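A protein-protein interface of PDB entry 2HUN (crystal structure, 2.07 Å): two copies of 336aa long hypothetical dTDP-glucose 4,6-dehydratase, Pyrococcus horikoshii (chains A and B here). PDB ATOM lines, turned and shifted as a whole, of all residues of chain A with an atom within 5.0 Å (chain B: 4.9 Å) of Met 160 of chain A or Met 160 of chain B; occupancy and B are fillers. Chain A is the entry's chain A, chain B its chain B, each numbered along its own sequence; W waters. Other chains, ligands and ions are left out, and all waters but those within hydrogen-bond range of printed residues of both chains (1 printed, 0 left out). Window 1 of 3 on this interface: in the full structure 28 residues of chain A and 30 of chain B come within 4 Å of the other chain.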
ATOM      1  N   LEU A 145       1.114 -27.700 -28.990  1.00  0.00           N
ATOM      2  CA  LEU A 145      -0.220 -28.261 -28.956  1.00  0.00           C
ATOM      3  C   LEU A 145      -0.662 -28.417 -30.410  1.00  0.00           C
ATOM      4  O   LEU A 145      -0.121 -27.760 -31.304  1.00  0.00           O
ATOM      5  CB  LEU A 145      -1.183 -27.326 -28.209  1.00  0.00           C
ATOM      6  CG  LEU A 145      -0.800 -26.973 -26.764  1.00  0.00           C
ATOM      7  CD1 LEU A 145      -1.920 -26.179 -26.114  1.00  0.00           C
ATOM      8  CD2 LEU A 145      -0.518 -28.225 -25.979  1.00  0.00           C
ATOM      9  N   PRO A 147      -4.507 -29.202 -31.345  1.00  0.00           N
ATOM     10  CA  PRO A 147      -5.910 -29.595 -31.169  1.00  0.00           C
ATOM     11  C   PRO A 147      -6.562 -29.950 -32.505  1.00  0.00           C
ATOM     12  O   PRO A 147      -6.350 -29.262 -33.500  1.00  0.00           O
ATOM     13  CB  PRO A 147      -6.531 -28.361 -30.527  1.00  0.00           C
ATOM     14  CG  PRO A 147      -5.740 -27.232 -31.151  1.00  0.00           C
ATOM     15  CD  PRO A 147      -4.321 -27.766 -31.058  1.00  0.00           C
ATOM     16  N   ALA A 153      -9.459 -27.309 -29.204  1.00  0.00           N
ATOM     17  CA  ALA A 153      -8.857 -26.041 -29.599  1.00  0.00           C
ATOM     18  C   ALA A 153      -9.243 -24.952 -28.599  1.00  0.00           C
ATOM     19  O   ALA A 153      -8.436 -24.057 -28.302  1.00  0.00           O
ATOM     20  CB  ALA A 153      -9.305 -25.653 -31.002  1.00  0.00           C
ATOM     21  N   ALA A 156      -7.364 -25.634 -25.430  1.00  0.00           N
ATOM     22  CA  ALA A 156      -5.983 -25.197 -25.670  1.00  0.00           C
ATOM     23  C   ALA A 156      -5.888 -23.684 -25.574  1.00  0.00           C
ATOM     24  O   ALA A 156      -4.953 -23.156 -24.981  1.00  0.00           O
ATOM     25  CB  ALA A 156      -5.502 -25.658 -27.050  1.00  0.00           C
ATOM     26  N   ALA A 157      -6.863 -22.993 -26.158  1.00  0.00           N
ATOM     27  CA  ALA A 157      -6.902 -21.539 -26.119  1.00  0.00           C
ATOM     28  C   ALA A 157      -7.010 -21.060 -24.680  1.00  0.00           C
ATOM     29  O   ALA A 157      -6.374 -20.072 -24.309  1.00  0.00           O
ATOM     30  CB  ALA A 157      -8.084 -21.013 -26.931  1.00  0.00           C
ATOM     31  N   SER A 158      -7.815 -21.747 -23.867  1.00  0.00           N
ATOM     32  CA  SER A 158      -7.963 -21.348 -22.472  1.00  0.00           C
ATOM     33  C   SER A 158      -6.646 -21.541 -21.723  1.00  0.00           C
ATOM     34  O   SER A 158      -6.290 -20.718 -20.882  1.00  0.00           O
ATOM     35  CB  SER A 158      -9.108 -22.114 -21.779  1.00  0.00           C
ATOM     36  OG  SER A 158      -8.819 -23.489 -21.595  1.00  0.00           O
ATOM     37  N   ASP A 159      -5.918 -22.615 -22.023  1.00  0.00           N
ATOM     38  CA  ASP A 159      -4.624 -22.844 -21.371  1.00  0.00           C
ATOM     39  C   ASP A 159      -3.702 -21.641 -21.618  1.00  0.00           C
ATOM     40  O   ASP A 159      -3.039 -21.148 -20.703  1.00  0.00           O
ATOM     41  CB  ASP A 159      -3.934 -24.102 -21.924  1.00  0.00           C
ATOM     42  CG  ASP A 159      -4.577 -25.390 -21.449  1.00  0.00           C
ATOM     43  OD1 ASP A 159      -5.613 -25.319 -20.762  1.00  0.00           O
ATOM     44  OD2 ASP A 159      -4.042 -26.479 -21.764  1.00  0.00           O
ATOM     45  N   MET A 160      -3.655 -21.178 -22.862  1.00  0.00           N
ATOM     46  CA  MET A 160      -2.798 -20.054 -23.222  1.00  0.00           C
ATOM     47  C   MET A 160      -3.124 -18.789 -22.425  1.00  0.00           C
ATOM     48  O   MET A 160      -2.210 -18.070 -21.992  1.00  0.00           O
ATOM     49  CB  MET A 160      -2.887 -19.768 -24.735  1.00  0.00           C
ATOM     50  CG  MET A 160      -2.374 -20.899 -25.625  1.00  0.00           C
ATOM     51  SD  MET A 160      -0.715 -21.492 -25.168  1.00  0.00           S
ATOM     52  CE  MET A 160      -1.087 -22.834 -24.107  1.00  0.00           C
ATOM     53  N   LEU A 161      -4.415 -18.510 -22.228  1.00  0.00           N
ATOM     54  CA  LEU A 161      -4.809 -17.323 -21.470  1.00  0.00           C
ATOM     55  C   LEU A 161      -4.307 -17.451 -20.039  1.00  0.00           C
ATOM     56  O   LEU A 161      -3.783 -16.496 -19.471  1.00  0.00           O
ATOM     57  CB  LEU A 161      -6.334 -17.146 -21.465  1.00  0.00           C
ATOM     58  CG  LEU A 161      -7.013 -16.981 -22.828  1.00  0.00           C
ATOM     59  CD1 LEU A 161      -8.506 -16.743 -22.628  1.00  0.00           C
ATOM     60  CD2 LEU A 161      -6.386 -15.826 -23.580  1.00  0.00           C
ATOM     61  N   VAL A 162      -4.455 -18.636 -19.457  1.00  0.00           N
ATOM     62  CA  VAL A 162      -3.993 -18.847 -18.093  1.00  0.00           C
ATOM     63  C   VAL A 162      -2.494 -18.587 -17.961  1.00  0.00           C
ATOM     64  O   VAL A 162      -2.058 -17.946 -17.011  1.00  0.00           O
ATOM     65  CB  VAL A 162      -4.307 -20.274 -17.600  1.00  0.00           C
ATOM     66  CG1 VAL A 162      -3.666 -20.512 -16.245  1.00  0.00           C
ATOM     67  CG2 VAL A 162      -5.810 -20.455 -17.492  1.00  0.00           C
ATOM     68  N   LEU A 163      -1.706 -19.084 -18.909  1.00  0.00           N
ATOM     69  CA  LEU A 163      -0.261 -18.883 -18.868  1.00  0.00           C
ATOM     70  C   LEU A 163       0.063 -17.388 -18.940  1.00  0.00           C
ATOM     71  O   LEU A 163       0.888 -16.883 -18.181  1.00  0.00           O
ATOM     72  CB  LEU A 163       0.407 -19.621 -20.031  1.00  0.00           C
ATOM     73  CG  LEU A 163       0.367 -21.158 -19.979  1.00  0.00           C
ATOM     74  CD1 LEU A 163       0.968 -21.747 -21.251  1.00  0.00           C
ATOM     75  CD2 LEU A 163       1.126 -21.645 -18.764  1.00  0.00           C
ATOM     76  N   GLY A 164      -0.614 -16.687 -19.842  1.00  0.00           N
ATOM     77  CA  GLY A 164      -0.385 -15.264 -20.019  1.00  0.00           C
ATOM     78  C   GLY A 164      -0.784 -14.400 -18.840  1.00  0.00           C
ATOM     79  O   GLY A 164      -0.009 -13.551 -18.397  1.00  0.00           O
ATOM     80  N   ARG A 177      -3.304 -31.437 -16.985  1.00  0.00           N
ATOM     81  CA  ARG A 177      -3.783 -32.086 -18.202  1.00  0.00           C
ATOM     82  C   ARG A 177      -3.784 -33.584 -17.930  1.00  0.00           C
ATOM     83  O   ARG A 177      -2.734 -34.185 -17.674  1.00  0.00           O
ATOM     84  CB  ARG A 177      -2.874 -31.751 -19.400  1.00  0.00           C
ATOM     85  CG  ARG A 177      -3.039 -30.327 -19.932  1.00  0.00           C
ATOM     86  CD  ARG A 177      -1.959 -29.978 -20.942  1.00  0.00           C
ATOM     87  NE  ARG A 177      -2.093 -28.621 -21.475  1.00  0.00           N
ATOM     88  CZ  ARG A 177      -1.097 -27.973 -22.078  1.00  0.00           C
ATOM     89  NH1 ARG A 177       0.085 -28.566 -22.211  1.00  0.00           N
ATOM     90  NH2 ARG A 177      -1.279 -26.746 -22.551  1.00  0.00           N
ATOM     91  N   LEU B 145       4.146 -23.049 -26.144  1.00  0.00           N
ATOM     92  CA  LEU B 145       4.058 -21.604 -26.097  1.00  0.00           C
ATOM     93  C   LEU B 145       4.097 -21.225 -24.618  1.00  0.00           C
ATOM     94  O   LEU B 145       3.840 -22.068 -23.757  1.00  0.00           O
ATOM     95  CB  LEU B 145       2.747 -21.121 -26.733  1.00  0.00           C
ATOM     96  CG  LEU B 145       2.490 -21.594 -28.171  1.00  0.00           C
ATOM     97  CD1 LEU B 145       1.282 -20.842 -28.746  1.00  0.00           C
ATOM     98  CD2 LEU B 145       3.718 -21.352 -29.038  1.00  0.00           C
ATOM     99  N   PRO B 147       3.215 -17.460 -23.490  1.00  0.00           N
ATOM    100  CA  PRO B 147       2.967 -16.017 -23.592  1.00  0.00           C
ATOM    101  C   PRO B 147       3.057 -15.327 -22.235  1.00  0.00           C
ATOM    102  O   PRO B 147       2.539 -15.837 -21.239  1.00  0.00           O
ATOM    103  CB  PRO B 147       1.563 -15.950 -24.194  1.00  0.00           C
ATOM    104  CG  PRO B 147       0.902 -17.145 -23.602  1.00  0.00           C
ATOM    105  CD  PRO B 147       1.981 -18.218 -23.761  1.00  0.00           C
ATOM    106  N   ALA B 153      -0.774 -13.727 -25.182  1.00  0.00           N
ATOM    107  CA  ALA B 153      -1.623 -14.830 -24.740  1.00  0.00           C
ATOM    108  C   ALA B 153      -2.841 -14.964 -25.653  1.00  0.00           C
ATOM    109  O   ALA B 153      -3.239 -16.077 -26.005  1.00  0.00           O
ATOM    110  CB  ALA B 153      -2.066 -14.602 -23.307  1.00  0.00           C
ATOM    111  N   ALA B 156      -1.717 -16.186 -28.906  1.00  0.00           N
ATOM    112  CA  ALA B 156      -1.469 -17.617 -28.780  1.00  0.00           C
ATOM    113  C   ALA B 156      -2.795 -18.378 -28.792  1.00  0.00           C
ATOM    114  O   ALA B 156      -2.894 -19.463 -29.357  1.00  0.00           O
ATOM    115  CB  ALA B 156      -0.701 -17.908 -27.494  1.00  0.00           C
ATOM    116  N   ALA B 157      -3.814 -17.802 -28.164  1.00  0.00           N
ATOM    117  CA  ALA B 157      -5.126 -18.433 -28.128  1.00  0.00           C
ATOM    118  C   ALA B 157      -5.672 -18.493 -29.551  1.00  0.00           C
ATOM    119  O   ALA B 157      -6.254 -19.504 -29.954  1.00  0.00           O
ATOM    120  CB  ALA B 157      -6.077 -17.641 -27.225  1.00  0.00           C
ATOM    121  N   SER B 158      -5.476 -17.414 -30.311  1.00  0.00           N
ATOM    122  CA  SER B 158      -5.948 -17.364 -31.695  1.00  0.00           C
ATOM    123  C   SER B 158      -5.247 -18.444 -32.533  1.00  0.00           C
ATOM    124  O   SER B 158      -5.891 -19.123 -33.334  1.00  0.00           O
ATOM    125  CB  SER B 158      -5.724 -15.973 -32.305  1.00  0.00           C
ATOM    126  OG  SER B 158      -4.350 -15.688 -32.507  1.00  0.00           O
ATOM    127  N   ASP B 159      -3.936 -18.609 -32.349  1.00  0.00           N
ATOM    128  CA  ASP B 159      -3.189 -19.643 -33.077  1.00  0.00           C
ATOM    129  C   ASP B 159      -3.852 -21.006 -32.875  1.00  0.00           C
ATOM    130  O   ASP B 159      -4.044 -21.764 -33.826  1.00  0.00           O
ATOM    131  CB  ASP B 159      -1.747 -19.767 -32.567  1.00  0.00           C
ATOM    132  CG  ASP B 159      -0.854 -18.626 -33.005  1.00  0.00           C
ATOM    133  OD1 ASP B 159      -1.335 -17.683 -33.663  1.00  0.00           O
ATOM    134  OD2 ASP B 159       0.347 -18.683 -32.672  1.00  0.00           O
ATOM    135  N   MET B 160      -4.161 -21.321 -31.620  1.00  0.00           N
ATOM    136  CA  MET B 160      -4.781 -22.597 -31.269  1.00  0.00           C
ATOM    137  C   MET B 160      -6.126 -22.814 -31.970  1.00  0.00           C
ATOM    138  O   MET B 160      -6.411 -23.910 -32.447  1.00  0.00           O
ATOM    139  CB  MET B 160      -4.955 -22.692 -29.751  1.00  0.00           C
ATOM    140  CG  MET B 160      -3.659 -22.605 -28.966  1.00  0.00           C
ATOM    141  SD  MET B 160      -2.518 -23.953 -29.341  1.00  0.00           S
ATOM    142  CE  MET B 160      -1.551 -23.214 -30.660  1.00  0.00           C
ATOM    143  N   LEU B 161      -6.959 -21.779 -32.020  1.00  0.00           N
ATOM    144  CA  LEU B 161      -8.248 -21.899 -32.693  1.00  0.00           C
ATOM    145  C   LEU B 161      -8.020 -22.235 -34.164  1.00  0.00           C
ATOM    146  O   LEU B 161      -8.679 -23.108 -34.717  1.00  0.00           O
ATOM    147  CB  LEU B 161      -9.052 -20.593 -32.578  1.00  0.00           C
ATOM    148  CG  LEU B 161      -9.431 -20.122 -31.165  1.00  0.00           C
ATOM    149  CD1 LEU B 161     -10.412 -18.945 -31.265  1.00  0.00           C
ATOM    150  CD2 LEU B 161     -10.066 -21.257 -30.378  1.00  0.00           C
ATOM    151  N   VAL B 162      -7.063 -21.553 -34.787  1.00  0.00           N
ATOM    152  CA  VAL B 162      -6.756 -21.788 -36.192  1.00  0.00           C
ATOM    153  C   VAL B 162      -6.350 -23.237 -36.440  1.00  0.00           C
ATOM    154  O   VAL B 162      -6.815 -23.865 -37.387  1.00  0.00           O
ATOM    155  CB  VAL B 162      -5.618 -20.847 -36.685  1.00  0.00           C
ATOM    156  CG1 VAL B 162      -5.201 -21.224 -38.108  1.00  0.00           C
ATOM    157  CG2 VAL B 162      -6.094 -19.393 -36.654  1.00  0.00           C
ATOM    158  N   LEU B 163      -5.482 -23.774 -35.590  1.00  0.00           N
ATOM    159  CA  LEU B 163      -5.035 -25.151 -35.756  1.00  0.00           C
ATOM    160  C   LEU B 163      -6.216 -26.120 -35.672  1.00  0.00           C
ATOM    161  O   LEU B 163      -6.388 -26.984 -36.539  1.00  0.00           O
ATOM    162  CB  LEU B 163      -3.997 -25.505 -34.690  1.00  0.00           C
ATOM    163  CG  LEU B 163      -2.665 -24.753 -34.736  1.00  0.00           C
ATOM    164  CD1 LEU B 163      -1.800 -25.184 -33.555  1.00  0.00           C
ATOM    165  CD2 LEU B 163      -1.953 -25.048 -36.052  1.00  0.00           C
ATOM    166  N   GLY B 164      -7.028 -25.957 -34.628  1.00  0.00           N
ATOM    167  CA  GLY B 164      -8.188 -26.811 -34.430  1.00  0.00           C
ATOM    168  C   GLY B 164      -9.198 -26.724 -35.565  1.00  0.00           C
ATOM    169  O   GLY B 164      -9.670 -27.748 -36.047  1.00  0.00           O
ATOM    170  N   ARG B 177       4.739 -16.930 -37.726  1.00  0.00           N
ATOM    171  CA  ARG B 177       5.169 -16.257 -36.509  1.00  0.00           C
ATOM    172  C   ARG B 177       6.510 -15.595 -36.817  1.00  0.00           C
ATOM    173  O   ARG B 177       7.528 -16.272 -36.992  1.00  0.00           O
ATOM    174  CB  ARG B 177       5.325 -17.262 -35.362  1.00  0.00           C
ATOM    175  CG  ARG B 177       4.003 -17.850 -34.870  1.00  0.00           C
ATOM    176  CD  ARG B 177       4.212 -19.043 -33.953  1.00  0.00           C
ATOM    177  NE  ARG B 177       2.941 -19.524 -33.409  1.00  0.00           N
ATOM    178  CZ  ARG B 177       2.782 -20.679 -32.779  1.00  0.00           C
ATOM    179  NH1 ARG B 177       3.817 -21.497 -32.606  1.00  0.00           N
ATOM    180  NH2 ARG B 177       1.584 -21.018 -32.318  1.00  0.00           N
HETATM  181  O   HOH W   1       1.531 -24.169 -26.254  1.00  0.00           O
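Of the 13 printed residues of chain A, 8 touch a printed residue of chain B.
Hydrophobic or aromatic side chains of chain A within 4 Å of the printed part of chain B: Leu 145, Pro 147, Ala 153, Ala 157, Met 160, Leu 161 and Leu 163.
Printed residues of chain B that touch a printed residue of chain A: Leu 145, Pro 147, Ala 153, Ala 156, Ala 157, Met 160, Leu 161, Leu 163 and Gly 164.
Water W1 bridges the backbone NH (N) of Leu 145 of chain B (2.8 Å) and the side-chain sulfur (SD) of Met 160 of chain A (3.7 Å).
SD of Met 160 of chain B touches CB of Leu 145 of chain A (3.8 Å).
O of Leu 145 of chain A touches CD1 of Leu 163 of chain B, 3.8 Å away.
O of Pro 147 of chain A touches CA of Gly 164 of chain B, at 3.2 Å.
Ala 153 of chain A touches Met 160 of chain B (CB to O, 3.7 Å).
CA of Gly 164 of chain B touches CB of Ala 153 of chain A, at 3.8 Å.
Met 160 of chain A touches Leu 145 of chain B.
O of Met 160 of chain A touches CB of Ala 153 of chain B, 3.7 Å away.
Leu 161 of chain A touches Ala 153 of chain B.
CD1 of Leu 163 of chain A touches O of Leu 145 of chain B, 3.8 Å away.
CA of Gly 164 of chain A touches O of Pro 147 of chain B, 3.2 Å away.
Leu 145 of chain A touches Leu 163 of chain B, and with the chains exchanged Leu 163 of chain A touches Leu 145 of chain B.
Pro 147 of chain A touches Gly 164 of chain B, and with the chains exchanged Gly 164 of chain A touches Pro 147 of chain B.
Ala 153 of chain A touches Leu 161 of chain B, and with the chains exchanged Leu 161 of chain A touches Ala 153 of chain B.
Ala 157 of chain A touches Leu 161 of chain B, but with the chains exchanged Leu 161 of chain A does not touch Ala 157 of chain B (4.1 Å).
Positions printed for both chains: 145, 147, 153, 156, 157, 158, 159, 160, 161, 162, 163, 164 and 177.
Of the 20 pairs that touch across the chains among the printed residues, 18 have their exchanged pair printed and touching as well.
Of the printed residues of chain B, Ala 157 of chain A touches Ala 157 and Leu 161.
Met 160 of chain A touches just these residues of chain B: Leu 145, Pro 147, Ala 153, Ala 156 and Met 160.
Of the printed residues of chain A, Pro 147 of chain B touches Met 160 (3.6 Å), Leu 163 (3.6 Å) and Gly 164 (3.2 Å).
Met 160 of chain B touches just these residues of chain A: Leu 145 (3.8 Å), Pro 147 (3.6 Å), Ala 153 (3.7 Å) and Met 160 (3.97 Å).
Of the printed residues of chain A, Leu 161 of chain B touches Ala 153 (3.8 Å) and Ala 157 (3.98 Å).
Of the printed residues of chain A, Leu 163 of chain B touches Leu 145 (3.8 Å) and Pro 147 (3.8 Å).
Printed residues of chain A within 4 Å of Gly 164 of chain B: Pro 147 and Ala 153.
The nearest residue of chain B that does not touch Met 160 of chain A is Ala 157 of chain B (4.1 Å).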
